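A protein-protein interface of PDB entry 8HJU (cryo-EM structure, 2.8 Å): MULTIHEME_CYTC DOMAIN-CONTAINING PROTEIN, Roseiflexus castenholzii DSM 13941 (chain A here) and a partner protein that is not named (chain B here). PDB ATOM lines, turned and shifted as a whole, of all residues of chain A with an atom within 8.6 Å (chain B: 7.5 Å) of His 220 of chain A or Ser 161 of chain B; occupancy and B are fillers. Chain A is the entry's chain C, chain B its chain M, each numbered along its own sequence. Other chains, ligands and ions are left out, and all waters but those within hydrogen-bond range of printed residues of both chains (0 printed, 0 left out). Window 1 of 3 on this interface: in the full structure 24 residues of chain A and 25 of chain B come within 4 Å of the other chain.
The side-chain hydroxyl (OG1) of Thr 88 of chain B sits close to the backbone NH (N) of Ser 218 of chain A, 3.4 Å away.
The side-chain amide nitrogen of Asn 219 of chain A sits at hydrogen-bond distance from the backbone carbonyl oxygen of Ala 162 of chain B (3.5 Å).
The side-chain hydroxyl of Ser 218 of chain A lies within hydrogen-bond range of the backbone NH of Ala 162 of chain B (3.1 Å).
The indole nitrogen of Trp 174 of chain B lies close to the side-chain amide nitrogen of Asn 219 of chain A.
The backbone carbonyl oxygen of Ser 161 of chain B lies close to the side-chain hydroxyl of Ser 218 of chain A, at 3.2 Å.
The side-chain amide nitrogen of Asn 219 of chain A is in hydrogen-bond range of the backbone carbonyl oxygen of Ser 161 of chain B.
The side-chain hydroxyl (OG1) of Thr 88 of chain B sits at hydrogen-bond distance from the side-chain carboxylate (OE2) of Glu 221 of chain A.
OD1 of Asn 225 of chain A is in hydrogen-bond range of NE2 of Gln 226 of chain A, 2.8 Å away.
NE2 of Gln 224 of chain A is in hydrogen-bond range of OE2 of Glu 223 of chain A (3.3 Å).
The backbone NH (N) of Asn 159 of chain B lies within hydrogen-bond range of the backbone carbonyl oxygen (O) of Pro 154 of chain B (3.3 Å).
The backbone NH of Ser 218 of chain A sits at hydrogen-bond distance from the side-chain carboxylate of Glu 221 of chain A (3.0 Å).
N of Ser 161 of chain B sits at hydrogen-bond distance from O of Pro 86 of chain B.
The backbone carbonyl oxygen of Ala 162 of chain B lies within hydrogen-bond range of the indole nitrogen of Trp 174 of chain B.
Among the printed residues, merely in contact across the chains: Ser 218 of chain A with Asn 159 of chain B (3.8 Å), Asn 219 of chain A with Tyr 177 of chain B (3.5 Å), Asn 219 of chain A with Val 178 of chain B (3.7 Å), His 220 of chain A with Ser 161 of chain B (3.5 Å), Val 222 of chain A with Tyr 177 of chain B (3.6 Å), Glu 223 of chain A with Tyr 177 of chain B (3.3 Å) and Gln 226 of chain A with Tyr 177 of chain B (3.6 Å).
His 220 of chain A touches just one residue of chain B: Ser 161 (3.5 Å).
Of the printed residues of chain A, Asn 159 of chain B touches Ser 218 (3.8 Å).
Of chain A, only Ser 218, Asn 219 and His 220 come within 4 Å of Ser 161 of chain B.
Of chain A, only Ser 218 and Asn 219 come within 4 Å of Ala 162 of chain B.
Of the printed residues of chain A, Tyr 177 of chain B touches Asn 219 (3.5 Å), Val 222 (3.6 Å), Glu 223 (3.3 Å) and Gln 226 (3.6 Å).
The nearest residue of chain B that does not touch His 220 of chain A is Thr 88 of chain B (4.2 Å).
The nearest residue of chain A that does not touch Ser 161 of chain B is Glu 221 of chain A (5.8 Å).
Of the 12 printed residues of chain A, 7 touch a printed residue of chain B.
Hydrophobic or aromatic side chains of chain A that line the printed part of chain B: His 220 and Val 222.
Of the 23 printed residues of chain B, 7 touch a printed residue of chain A.
Hydrophobic or aromatic side chains of chain B within 4 Å of the printed part of chain A: Ala 162, Trp 174, Tyr 177 and Val 178.
Among the printed residues, 14 pairs touch across the chains.
Among the printed residues, no Asp or Glu carboxylate lies within 4 Å of a Lys or Arg side-chain nitrogen of the other chain.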
ATOM      1  N   VAL A 211     -12.725   4.771 -36.237  1.00  0.00           N
ATOM      2  CA  VAL A 211     -12.964   5.757 -35.190  1.00  0.00           C
ATOM      3  C   VAL A 211     -12.169   7.041 -35.363  1.00  0.00           C
ATOM      4  O   VAL A 211     -12.497   8.049 -34.719  1.00  0.00           O
ATOM      5  CB  VAL A 211     -12.674   5.126 -33.809  1.00  0.00           C
ATOM      6  CG1 VAL A 211     -11.220   4.729 -33.695  1.00  0.00           C
ATOM      7  CG2 VAL A 211     -13.072   6.059 -32.709  1.00  0.00           C
ATOM      8  N   VAL A 217     -18.454  10.316 -33.288  1.00  0.00           N
ATOM      9  CA  VAL A 217     -18.284   9.346 -32.222  1.00  0.00           C
ATOM     10  C   VAL A 217     -17.453  10.005 -31.130  1.00  0.00           C
ATOM     11  O   VAL A 217     -16.870  11.070 -31.320  1.00  0.00           O
ATOM     12  CB  VAL A 217     -17.617   8.047 -32.713  1.00  0.00           C
ATOM     13  CG1 VAL A 217     -18.377   7.482 -33.891  1.00  0.00           C
ATOM     14  CG2 VAL A 217     -16.176   8.298 -33.088  1.00  0.00           C
ATOM     15  N   SER A 218     -17.381   9.357 -29.971  1.00  0.00           N
ATOM     16  CA  SER A 218     -16.533   9.858 -28.894  1.00  0.00           C
ATOM     17  C   SER A 218     -15.903   8.679 -28.206  1.00  0.00           C
ATOM     18  O   SER A 218     -15.883   7.584 -28.755  1.00  0.00           O
ATOM     19  CB  SER A 218     -17.314  10.664 -27.873  1.00  0.00           C
ATOM     20  OG  SER A 218     -16.474  11.089 -26.832  1.00  0.00           O
ATOM     21  N   ASN A 219     -15.428   8.882 -26.988  1.00  0.00           N
ATOM     22  CA  ASN A 219     -14.714   7.819 -26.290  1.00  0.00           C
ATOM     23  C   ASN A 219     -15.495   6.528 -26.047  1.00  0.00           C
ATOM     24  O   ASN A 219     -14.885   5.499 -25.790  1.00  0.00           O
ATOM     25  CB  ASN A 219     -14.117   8.344 -24.985  1.00  0.00           C
ATOM     26  CG  ASN A 219     -13.071   9.417 -25.212  1.00  0.00           C
ATOM     27  OD1 ASN A 219     -12.479   9.498 -26.284  1.00  0.00           O
ATOM     28  ND2 ASN A 219     -12.835  10.243 -24.199  1.00  0.00           N
ATOM     29  N   HIS A 220     -16.822   6.562 -26.123  1.00  0.00           N
ATOM     30  CA  HIS A 220     -17.584   5.327 -25.978  1.00  0.00           C
ATOM     31  C   HIS A 220     -17.359   4.402 -27.173  1.00  0.00           C
ATOM     32  O   HIS A 220     -17.112   3.196 -27.009  1.00  0.00           O
ATOM     33  CB  HIS A 220     -19.060   5.673 -25.803  1.00  0.00           C
ATOM     34  CG  HIS A 220     -19.950   4.484 -25.620  1.00  0.00           C
ATOM     35  ND1 HIS A 220     -20.870   4.093 -26.568  1.00  0.00           N
ATOM     36  CD2 HIS A 220     -20.074   3.611 -24.593  1.00  0.00           C
ATOM     37  CE1 HIS A 220     -21.514   3.025 -26.138  1.00  0.00           C
ATOM     38  NE2 HIS A 220     -21.052   2.713 -24.941  1.00  0.00           N
ATOM     39  N   GLU A 221     -17.394   4.957 -28.383  1.00  0.00           N
ATOM     40  CA  GLU A 221     -17.095   4.167 -29.568  1.00  0.00           C
ATOM     41  C   GLU A 221     -15.620   3.798 -29.630  1.00  0.00           C
ATOM     42  O   GLU A 221     -15.271   2.708 -30.092  1.00  0.00           O
ATOM     43  CB  GLU A 221     -17.510   4.928 -30.821  1.00  0.00           C
ATOM     44  CG  GLU A 221     -19.005   4.983 -31.033  1.00  0.00           C
ATOM     45  CD  GLU A 221     -19.698   5.931 -30.078  1.00  0.00           C
ATOM     46  OE1 GLU A 221     -20.855   5.657 -29.705  1.00  0.00           O
ATOM     47  OE2 GLU A 221     -19.089   6.949 -29.700  1.00  0.00           O
ATOM     48  N   VAL A 222     -14.737   4.689 -29.175  1.00  0.00           N
ATOM     49  CA  VAL A 222     -13.324   4.336 -29.106  1.00  0.00           C
ATOM     50  C   VAL A 222     -13.109   3.196 -28.126  1.00  0.00           C
ATOM     51  O   VAL A 222     -12.264   2.328 -28.349  1.00  0.00           O
ATOM     52  CB  VAL A 222     -12.465   5.558 -28.733  1.00  0.00           C
ATOM     53  CG1 VAL A 222     -11.013   5.274 -29.031  1.00  0.00           C
ATOM     54  CG2 VAL A 222     -12.925   6.781 -29.479  1.00  0.00           C
ATOM     55  N   GLU A 223     -13.880   3.161 -27.044  1.00  0.00           N
ATOM     56  CA  GLU A 223     -13.773   2.070 -26.084  1.00  0.00           C
ATOM     57  C   GLU A 223     -14.252   0.754 -26.681  1.00  0.00           C
ATOM     58  O   GLU A 223     -13.636  -0.294 -26.463  1.00  0.00           O
ATOM     59  CB  GLU A 223     -14.567   2.414 -24.831  1.00  0.00           C
ATOM     60  CG  GLU A 223     -14.515   1.372 -23.750  1.00  0.00           C
ATOM     61  CD  GLU A 223     -15.621   1.553 -22.738  1.00  0.00           C
ATOM     62  OE1 GLU A 223     -15.356   1.406 -21.530  1.00  0.00           O
ATOM     63  OE2 GLU A 223     -16.761   1.845 -23.154  1.00  0.00           O
ATOM     64  N   GLN A 224     -15.352   0.783 -27.433  1.00  0.00           N
ATOM     65  CA  GLN A 224     -15.797  -0.432 -28.113  1.00  0.00           C
ATOM     66  C   GLN A 224     -14.763  -0.911 -29.125  1.00  0.00           C
ATOM     67  O   GLN A 224     -14.468  -2.115 -29.220  1.00  0.00           O
ATOM     68  CB  GLN A 224     -17.138  -0.185 -28.793  1.00  0.00           C
ATOM     69  CG  GLN A 224     -18.244   0.161 -27.828  1.00  0.00           C
ATOM     70  CD  GLN A 224     -18.210  -0.699 -26.585  1.00  0.00           C
ATOM     71  OE1 GLN A 224     -18.234  -1.924 -26.665  1.00  0.00           O
ATOM     72  NE2 GLN A 224     -18.147  -0.059 -25.426  1.00  0.00           N
ATOM     73  N   ASN A 225     -14.207   0.024 -29.894  1.00  0.00           N
ATOM     74  CA  ASN A 225     -13.143  -0.297 -30.831  1.00  0.00           C
ATOM     75  C   ASN A 225     -11.960  -0.932 -30.118  1.00  0.00           C
ATOM     76  O   ASN A 225     -11.386  -1.909 -30.604  1.00  0.00           O
ATOM     77  CB  ASN A 225     -12.727   0.979 -31.566  1.00  0.00           C
ATOM     78  CG  ASN A 225     -11.437   0.830 -32.328  1.00  0.00           C
ATOM     79  OD1 ASN A 225     -10.360   1.047 -31.789  1.00  0.00           O
ATOM     80  ND2 ASN A 225     -11.537   0.438 -33.583  1.00  0.00           N
ATOM     81  N   GLN A 226     -11.597  -0.407 -28.949  1.00  0.00           N
ATOM     82  CA  GLN A 226     -10.439  -0.921 -28.233  1.00  0.00           C
ATOM     83  C   GLN A 226     -10.711  -2.287 -27.629  1.00  0.00           C
ATOM     84  O   GLN A 226      -9.798  -3.109 -27.532  1.00  0.00           O
ATOM     85  CB  GLN A 226     -10.015   0.067 -27.154  1.00  0.00           C
ATOM     86  CG  GLN A 226      -9.332   1.286 -27.712  1.00  0.00           C
ATOM     87  CD  GLN A 226      -8.178   0.921 -28.602  1.00  0.00           C
ATOM     88  OE1 GLN A 226      -7.189   0.351 -28.158  1.00  0.00           O
ATOM     89  NE2 GLN A 226      -8.295   1.256 -29.869  1.00  0.00           N
ATOM     90  N   PHE A 227     -11.953  -2.557 -27.231  1.00  0.00           N
ATOM     91  CA  PHE A 227     -12.304  -3.906 -26.798  1.00  0.00           C
ATOM     92  C   PHE A 227     -12.133  -4.898 -27.937  1.00  0.00           C
ATOM     93  O   PHE A 227     -11.523  -5.960 -27.767  1.00  0.00           O
ATOM     94  CB  PHE A 227     -13.735  -3.939 -26.273  1.00  0.00           C
ATOM     95  CG  PHE A 227     -13.919  -3.223 -24.979  1.00  0.00           C
ATOM     96  CD1 PHE A 227     -12.852  -3.020 -24.131  1.00  0.00           C
ATOM     97  CD2 PHE A 227     -15.160  -2.752 -24.608  1.00  0.00           C
ATOM     98  CE1 PHE A 227     -13.018  -2.360 -22.942  1.00  0.00           C
ATOM     99  CE2 PHE A 227     -15.327  -2.091 -23.422  1.00  0.00           C
ATOM    100  CZ  PHE A 227     -14.253  -1.896 -22.587  1.00  0.00           C
ATOM    101  N   TYR B  84     -18.622   6.509 -15.731  1.00  0.00           N
ATOM    102  CA  TYR B  84     -18.335   7.095 -17.025  1.00  0.00           C
ATOM    103  C   TYR B  84     -19.320   8.209 -17.358  1.00  0.00           C
ATOM    104  O   TYR B  84     -20.464   8.190 -16.904  1.00  0.00           O
ATOM    105  CB  TYR B  84     -18.372   6.024 -18.103  1.00  0.00           C
ATOM    106  CG  TYR B  84     -17.177   5.117 -18.036  1.00  0.00           C
ATOM    107  CD1 TYR B  84     -16.017   5.421 -18.725  1.00  0.00           C
ATOM    108  CD2 TYR B  84     -17.196   3.973 -17.263  1.00  0.00           C
ATOM    109  CE1 TYR B  84     -14.917   4.605 -18.659  1.00  0.00           C
ATOM    110  CE2 TYR B  84     -16.104   3.149 -17.190  1.00  0.00           C
ATOM    111  CZ  TYR B  84     -14.964   3.467 -17.888  1.00  0.00           C
ATOM    112  OH  TYR B  84     -13.866   2.644 -17.816  1.00  0.00           O
ATOM    113  N   PRO B  85     -18.889   9.197 -18.136  1.00  0.00           N
ATOM    114  CA  PRO B  85     -19.788  10.268 -18.549  1.00  0.00           C
ATOM    115  C   PRO B  85     -20.898   9.728 -19.430  1.00  0.00           C
ATOM    116  O   PRO B  85     -20.837   8.575 -19.875  1.00  0.00           O
ATOM    117  CB  PRO B  85     -18.866  11.219 -19.326  1.00  0.00           C
ATOM    118  CG  PRO B  85     -17.718  10.402 -19.716  1.00  0.00           C
ATOM    119  CD  PRO B  85     -17.520   9.426 -18.615  1.00  0.00           C
ATOM    120  N   PRO B  86     -21.936  10.517 -19.688  1.00  0.00           N
ATOM    121  CA  PRO B  86     -23.013  10.058 -20.559  1.00  0.00           C
ATOM    122  C   PRO B  86     -22.478   9.653 -21.917  1.00  0.00           C
ATOM    123  O   PRO B  86     -21.536  10.274 -22.428  1.00  0.00           O
ATOM    124  CB  PRO B  86     -23.924  11.286 -20.665  1.00  0.00           C
ATOM    125  CG  PRO B  86     -23.669  12.033 -19.433  1.00  0.00           C
ATOM    126  CD  PRO B  86     -22.233  11.831 -19.100  1.00  0.00           C
ATOM    127  N   PRO B  87     -23.039   8.611 -22.528  1.00  0.00           N
ATOM    128  CA  PRO B  87     -22.556   8.177 -23.844  1.00  0.00           C
ATOM    129  C   PRO B  87     -22.754   9.229 -24.920  1.00  0.00           C
ATOM    130  O   PRO B  87     -23.354  10.277 -24.672  1.00  0.00           O
ATOM    131  CB  PRO B  87     -23.392   6.926 -24.124  1.00  0.00           C
ATOM    132  CG  PRO B  87     -23.846   6.469 -22.790  1.00  0.00           C
ATOM    133  CD  PRO B  87     -24.058   7.700 -21.990  1.00  0.00           C
ATOM    134  N   THR B  88     -22.250   8.953 -26.124  1.00  0.00           N
ATOM    135  CA  THR B  88     -22.285   9.946 -27.192  1.00  0.00           C
ATOM    136  C   THR B  88     -23.713  10.302 -27.580  1.00  0.00           C
ATOM    137  O   THR B  88     -24.009  11.463 -27.880  1.00  0.00           O
ATOM    138  CB  THR B  88     -21.513   9.435 -28.402  1.00  0.00           C
ATOM    139  OG1 THR B  88     -20.178   9.116 -28.004  1.00  0.00           O
ATOM    140  CG2 THR B  88     -21.462  10.496 -29.486  1.00  0.00           C
ATOM    141  N   GLU B  89     -24.614   9.322 -27.554  1.00  0.00           N
ATOM    142  CA  GLU B  89     -26.024   9.606 -27.814  1.00  0.00           C
ATOM    143  C   GLU B  89     -26.468  10.492 -26.670  1.00  0.00           C
ATOM    144  O   GLU B  89     -26.001  10.302 -25.553  1.00  0.00           O
ATOM    145  CB  GLU B  89     -26.828   8.312 -27.834  1.00  0.00           C
ATOM    146  CG  GLU B  89     -26.432   7.323 -26.750  1.00  0.00           C
ATOM    147  CD  GLU B  89     -27.446   6.216 -26.568  1.00  0.00           C
ATOM    148  OE1 GLU B  89     -28.508   6.269 -27.221  1.00  0.00           O
ATOM    149  OE2 GLU B  89     -27.187   5.297 -25.763  1.00  0.00           O
ATOM    150  N   TYR B  90     -27.323  11.482 -26.924  1.00  0.00           N
ATOM    151  CA  TYR B  90     -27.700  12.446 -25.872  1.00  0.00           C
ATOM    152  C   TYR B  90     -26.421  12.968 -25.245  1.00  0.00           C
ATOM    153  O   TYR B  90     -26.300  13.025 -24.025  1.00  0.00           O
ATOM    154  CB  TYR B  90     -28.770  11.949 -24.854  1.00  0.00           C
ATOM    155  CG  TYR B  90     -28.440  10.757 -23.965  1.00  0.00           C
ATOM    156  CD1 TYR B  90     -27.826  10.930 -22.731  1.00  0.00           C
ATOM    157  CD2 TYR B  90     -28.784   9.467 -24.343  1.00  0.00           C
ATOM    158  CE1 TYR B  90     -27.531   9.853 -21.918  1.00  0.00           C
ATOM    159  CE2 TYR B  90     -28.498   8.385 -23.533  1.00  0.00           C
ATOM    160  CZ  TYR B  90     -27.871   8.584 -22.322  1.00  0.00           C
ATOM    161  OH  TYR B  90     -27.584   7.511 -21.511  1.00  0.00           O
ATOM    162  N   GLY B  91     -25.464  13.367 -26.077  1.00  0.00           N
ATOM    163  CA  GLY B  91     -24.163  13.741 -25.554  1.00  0.00           C
ATOM    164  C   GLY B  91     -23.948  14.882 -24.592  1.00  0.00           C
ATOM    165  O   GLY B  91     -23.262  14.675 -23.606  1.00  0.00           O
ATOM    166  N   LEU B  92     -24.535  16.048 -24.802  1.00  0.00           N
ATOM    167  CA  LEU B  92     -24.319  17.096 -23.821  1.00  0.00           C
ATOM    168  C   LEU B  92     -25.459  17.163 -22.833  1.00  0.00           C
ATOM    169  O   LEU B  92     -25.359  17.869 -21.836  1.00  0.00           O
ATOM    170  CB  LEU B  92     -24.101  18.452 -24.485  1.00  0.00           C
ATOM    171  CG  LEU B  92     -22.663  18.801 -24.863  1.00  0.00           C
ATOM    172  CD1 LEU B  92     -22.599  20.180 -25.498  1.00  0.00           C
ATOM    173  CD2 LEU B  92     -21.737  18.718 -23.661  1.00  0.00           C
ATOM    174  N   TRP B 104     -21.966  10.764 -13.191  1.00  0.00           N
ATOM    175  CA  TRP B 104     -20.755  11.461 -13.599  1.00  0.00           C
ATOM    176  C   TRP B 104     -20.971  12.964 -13.647  1.00  0.00           C
ATOM    177  O   TRP B 104     -20.082  13.734 -13.274  1.00  0.00           O
ATOM    178  CB  TRP B 104     -20.285  10.948 -14.957  1.00  0.00           C
ATOM    179  CG  TRP B 104     -19.003  11.561 -15.405  1.00  0.00           C
ATOM    180  CD1 TRP B 104     -17.752  11.080 -15.189  1.00  0.00           C
ATOM    181  CD2 TRP B 104     -18.843  12.774 -16.142  1.00  0.00           C
ATOM    182  NE1 TRP B 104     -16.823  11.913 -15.745  1.00  0.00           N
ATOM    183  CE2 TRP B 104     -17.469  12.963 -16.337  1.00  0.00           C
ATOM    184  CE3 TRP B 104     -19.731  13.718 -16.659  1.00  0.00           C
ATOM    185  CZ2 TRP B 104     -16.963  14.052 -17.021  1.00  0.00           C
ATOM    186  CZ3 TRP B 104     -19.226  14.795 -17.332  1.00  0.00           C
ATOM    187  CH2 TRP B 104     -17.855  14.956 -17.512  1.00  0.00           C
ATOM    188  N   PRO B 154     -15.270  18.670 -23.836  1.00  0.00           N
ATOM    189  CA  PRO B 154     -16.553  17.985 -24.076  1.00  0.00           C
ATOM    190  C   PRO B 154     -17.575  18.880 -24.746  1.00  0.00           C
ATOM    191  O   PRO B 154     -18.131  18.514 -25.786  1.00  0.00           O
ATOM    192  CB  PRO B 154     -16.979  17.560 -22.672  1.00  0.00           C
ATOM    193  CG  PRO B 154     -15.732  17.372 -21.971  1.00  0.00           C
ATOM    194  CD  PRO B 154     -14.799  18.423 -22.465  1.00  0.00           C
ATOM    195  N   LEU B 157     -17.287  19.911 -28.552  1.00  0.00           N
ATOM    196  CA  LEU B 157     -17.346  18.653 -29.272  1.00  0.00           C
ATOM    197  C   LEU B 157     -18.754  18.097 -29.332  1.00  0.00           C
ATOM    198  O   LEU B 157     -19.044  17.283 -30.211  1.00  0.00           O
ATOM    199  CB  LEU B 157     -16.423  17.609 -28.630  1.00  0.00           C
ATOM    200  CG  LEU B 157     -14.932  17.679 -28.953  1.00  0.00           C
ATOM    201  CD1 LEU B 157     -14.200  16.565 -28.256  1.00  0.00           C
ATOM    202  CD2 LEU B 157     -14.688  17.619 -30.437  1.00  0.00           C
ATOM    203  N   GLY B 158     -19.629  18.524 -28.427  1.00  0.00           N
ATOM    204  CA  GLY B 158     -21.022  18.162 -28.462  1.00  0.00           C
ATOM    205  C   GLY B 158     -21.412  16.984 -27.607  1.00  0.00           C
ATOM    206  O   GLY B 158     -22.581  16.590 -27.633  1.00  0.00           O
ATOM    207  N   ASN B 159     -20.484  16.405 -26.856  1.00  0.00           N
ATOM    208  CA  ASN B 159     -20.792  15.229 -26.061  1.00  0.00           C
ATOM    209  C   ASN B 159     -19.970  15.230 -24.786  1.00  0.00           C
ATOM    210  O   ASN B 159     -18.803  15.625 -24.787  1.00  0.00           O
ATOM    211  CB  ASN B 159     -20.535  13.936 -26.843  1.00  0.00           C
ATOM    212  CG  ASN B 159     -19.299  14.007 -27.697  1.00  0.00           C
ATOM    213  OD1 ASN B 159     -18.235  14.395 -27.236  1.00  0.00           O
ATOM    214  ND2 ASN B 159     -19.433  13.629 -28.956  1.00  0.00           N
ATOM    215  N   TRP B 160     -20.594  14.783 -23.698  1.00  0.00           N
ATOM    216  CA  TRP B 160     -19.872  14.589 -22.452  1.00  0.00           C
ATOM    217  C   TRP B 160     -18.920  13.411 -22.523  1.00  0.00           C
ATOM    218  O   TRP B 160     -17.955  13.366 -21.756  1.00  0.00           O
ATOM    219  CB  TRP B 160     -20.852  14.382 -21.303  1.00  0.00           C
ATOM    220  CG  TRP B 160     -21.527  15.621 -20.872  1.00  0.00           C
ATOM    221  CD1 TRP B 160     -22.858  15.869 -20.885  1.00  0.00           C
ATOM    222  CD2 TRP B 160     -20.903  16.796 -20.353  1.00  0.00           C
ATOM    223  NE1 TRP B 160     -23.108  17.124 -20.408  1.00  0.00           N
ATOM    224  CE2 TRP B 160     -21.921  17.716 -20.073  1.00  0.00           C
ATOM    225  CE3 TRP B 160     -19.578  17.157 -20.096  1.00  0.00           C
ATOM    226  CZ2 TRP B 160     -21.663  18.973 -19.551  1.00  0.00           C
ATOM    227  CZ3 TRP B 160     -19.326  18.405 -19.579  1.00  0.00           C
ATOM    228  CH2 TRP B 160     -20.360  19.299 -19.312  1.00  0.00           C
ATOM    229  N   SER B 161     -19.165  12.466 -23.429  1.00  0.00           N
ATOM    230  CA  SER B 161     -18.318  11.287 -23.543  1.00  0.00           C
ATOM    231  C   SER B 161     -16.879  11.634 -23.879  1.00  0.00           C
ATOM    232  O   SER B 161     -15.999  10.786 -23.717  1.00  0.00           O
ATOM    233  CB  SER B 161     -18.882  10.346 -24.598  1.00  0.00           C
ATOM    234  OG  SER B 161     -18.552   9.011 -24.293  1.00  0.00           O
ATOM    235  N   ALA B 162     -16.615  12.857 -24.331  1.00  0.00           N
ATOM    236  CA  ALA B 162     -15.251  13.280 -24.601  1.00  0.00           C
ATOM    237  C   ALA B 162     -14.431  13.444 -23.333  1.00  0.00           C
ATOM    238  O   ALA B 162     -13.213  13.613 -23.420  1.00  0.00           O
ATOM    239  CB  ALA B 162     -15.261  14.589 -25.385  1.00  0.00           C
ATOM    240  N   ALA B 163     -15.061  13.399 -22.171  1.00  0.00           N
ATOM    241  CA  ALA B 163     -14.407  13.618 -20.894  1.00  0.00           C
ATOM    242  C   ALA B 163     -14.065  12.295 -20.221  1.00  0.00           C
ATOM    243  O   ALA B 163     -14.639  11.253 -20.543  1.00  0.00           O
ATOM    244  CB  ALA B 163     -15.308  14.453 -19.992  1.00  0.00           C
ATOM    245  N   PRO B 164     -13.119  12.300 -19.283  1.00  0.00           N
ATOM    246  CA  PRO B 164     -12.711  11.053 -18.626  1.00  0.00           C
ATOM    247  C   PRO B 164     -13.801  10.490 -17.729  1.00  0.00           C
ATOM    248  O   PRO B 164     -14.774  11.154 -17.375  1.00  0.00           O
ATOM    249  CB  PRO B 164     -11.485  11.464 -17.811  1.00  0.00           C
ATOM    250  CG  PRO B 164     -11.029  12.708 -18.420  1.00  0.00           C
ATOM    251  CD  PRO B 164     -12.217  13.406 -18.942  1.00  0.00           C
ATOM    252  N   GLY B 165     -13.601   9.239 -17.332  1.00  0.00           N
ATOM    253  CA  GLY B 165     -14.642   8.487 -16.669  1.00  0.00           C
ATOM    254  C   GLY B 165     -14.515   8.268 -15.175  1.00  0.00           C
ATOM    255  O   GLY B 165     -15.124   7.333 -14.656  1.00  0.00           O
ATOM    256  N   TRP B 174      -8.978   7.065 -20.909  1.00  0.00           N
ATOM    257  CA  TRP B 174      -9.367   8.305 -21.567  1.00  0.00           C
ATOM    258  C   TRP B 174      -8.229   8.863 -22.403  1.00  0.00           C
ATOM    259  O   TRP B 174      -8.442   9.315 -23.530  1.00  0.00           O
ATOM    260  CB  TRP B 174      -9.812   9.346 -20.548  1.00  0.00           C
ATOM    261  CG  TRP B 174     -10.080  10.676 -21.183  1.00  0.00           C
ATOM    262  CD1 TRP B 174     -11.250  11.095 -21.719  1.00  0.00           C
ATOM    263  CD2 TRP B 174      -9.149  11.750 -21.366  1.00  0.00           C
ATOM    264  NE1 TRP B 174     -11.118  12.361 -22.217  1.00  0.00           N
ATOM    265  CE2 TRP B 174      -9.836  12.788 -22.010  1.00  0.00           C
ATOM    266  CE3 TRP B 174      -7.804  11.933 -21.045  1.00  0.00           C
ATOM    267  CZ2 TRP B 174      -9.225  13.988 -22.344  1.00  0.00           C
ATOM    268  CZ3 TRP B 174      -7.205  13.120 -21.375  1.00  0.00           C
ATOM    269  CH2 TRP B 174      -7.911  14.134 -22.018  1.00  0.00           C
ATOM    270  N   TYR B 177      -7.872   6.746 -25.499  1.00  0.00           N
ATOM    271  CA  TYR B 177      -8.972   6.924 -26.439  1.00  0.00           C
ATOM    272  C   TYR B 177      -8.897   8.271 -27.132  1.00  0.00           C
ATOM    273  O   TYR B 177      -9.261   8.386 -28.301  1.00  0.00           O
ATOM    274  CB  TYR B 177     -10.316   6.799 -25.730  1.00  0.00           C
ATOM    275  CG  TYR B 177     -10.573   5.486 -25.045  1.00  0.00           C
ATOM    276  CD1 TYR B 177      -9.878   4.348 -25.398  1.00  0.00           C
ATOM    277  CD2 TYR B 177     -11.515   5.393 -24.039  1.00  0.00           C
ATOM    278  CE1 TYR B 177     -10.112   3.159 -24.771  1.00  0.00           C
ATOM    279  CE2 TYR B 177     -11.754   4.209 -23.406  1.00  0.00           C
ATOM    280  CZ  TYR B 177     -11.050   3.092 -23.776  1.00  0.00           C
ATOM    281  OH  TYR B 177     -11.287   1.898 -23.145  1.00  0.00           O
ATOM    282  N   VAL B 178      -8.459   9.308 -26.424  1.00  0.00           N
ATOM    283  CA  VAL B 178      -8.422  10.629 -27.034  1.00  0.00           C
ATOM    284  C   VAL B 178      -7.281  10.722 -28.031  1.00  0.00           C
ATOM    285  O   VAL B 178      -7.430  11.319 -29.101  1.00  0.00           O
ATOM    286  CB  VAL B 178      -8.341  11.723 -25.957  1.00  0.00           C
ATOM    287  CG1 VAL B 178      -8.076  13.063 -26.594  1.00  0.00           C
ATOM    288  CG2 VAL B 178      -9.630  11.777 -25.192  1.00  0.00           C
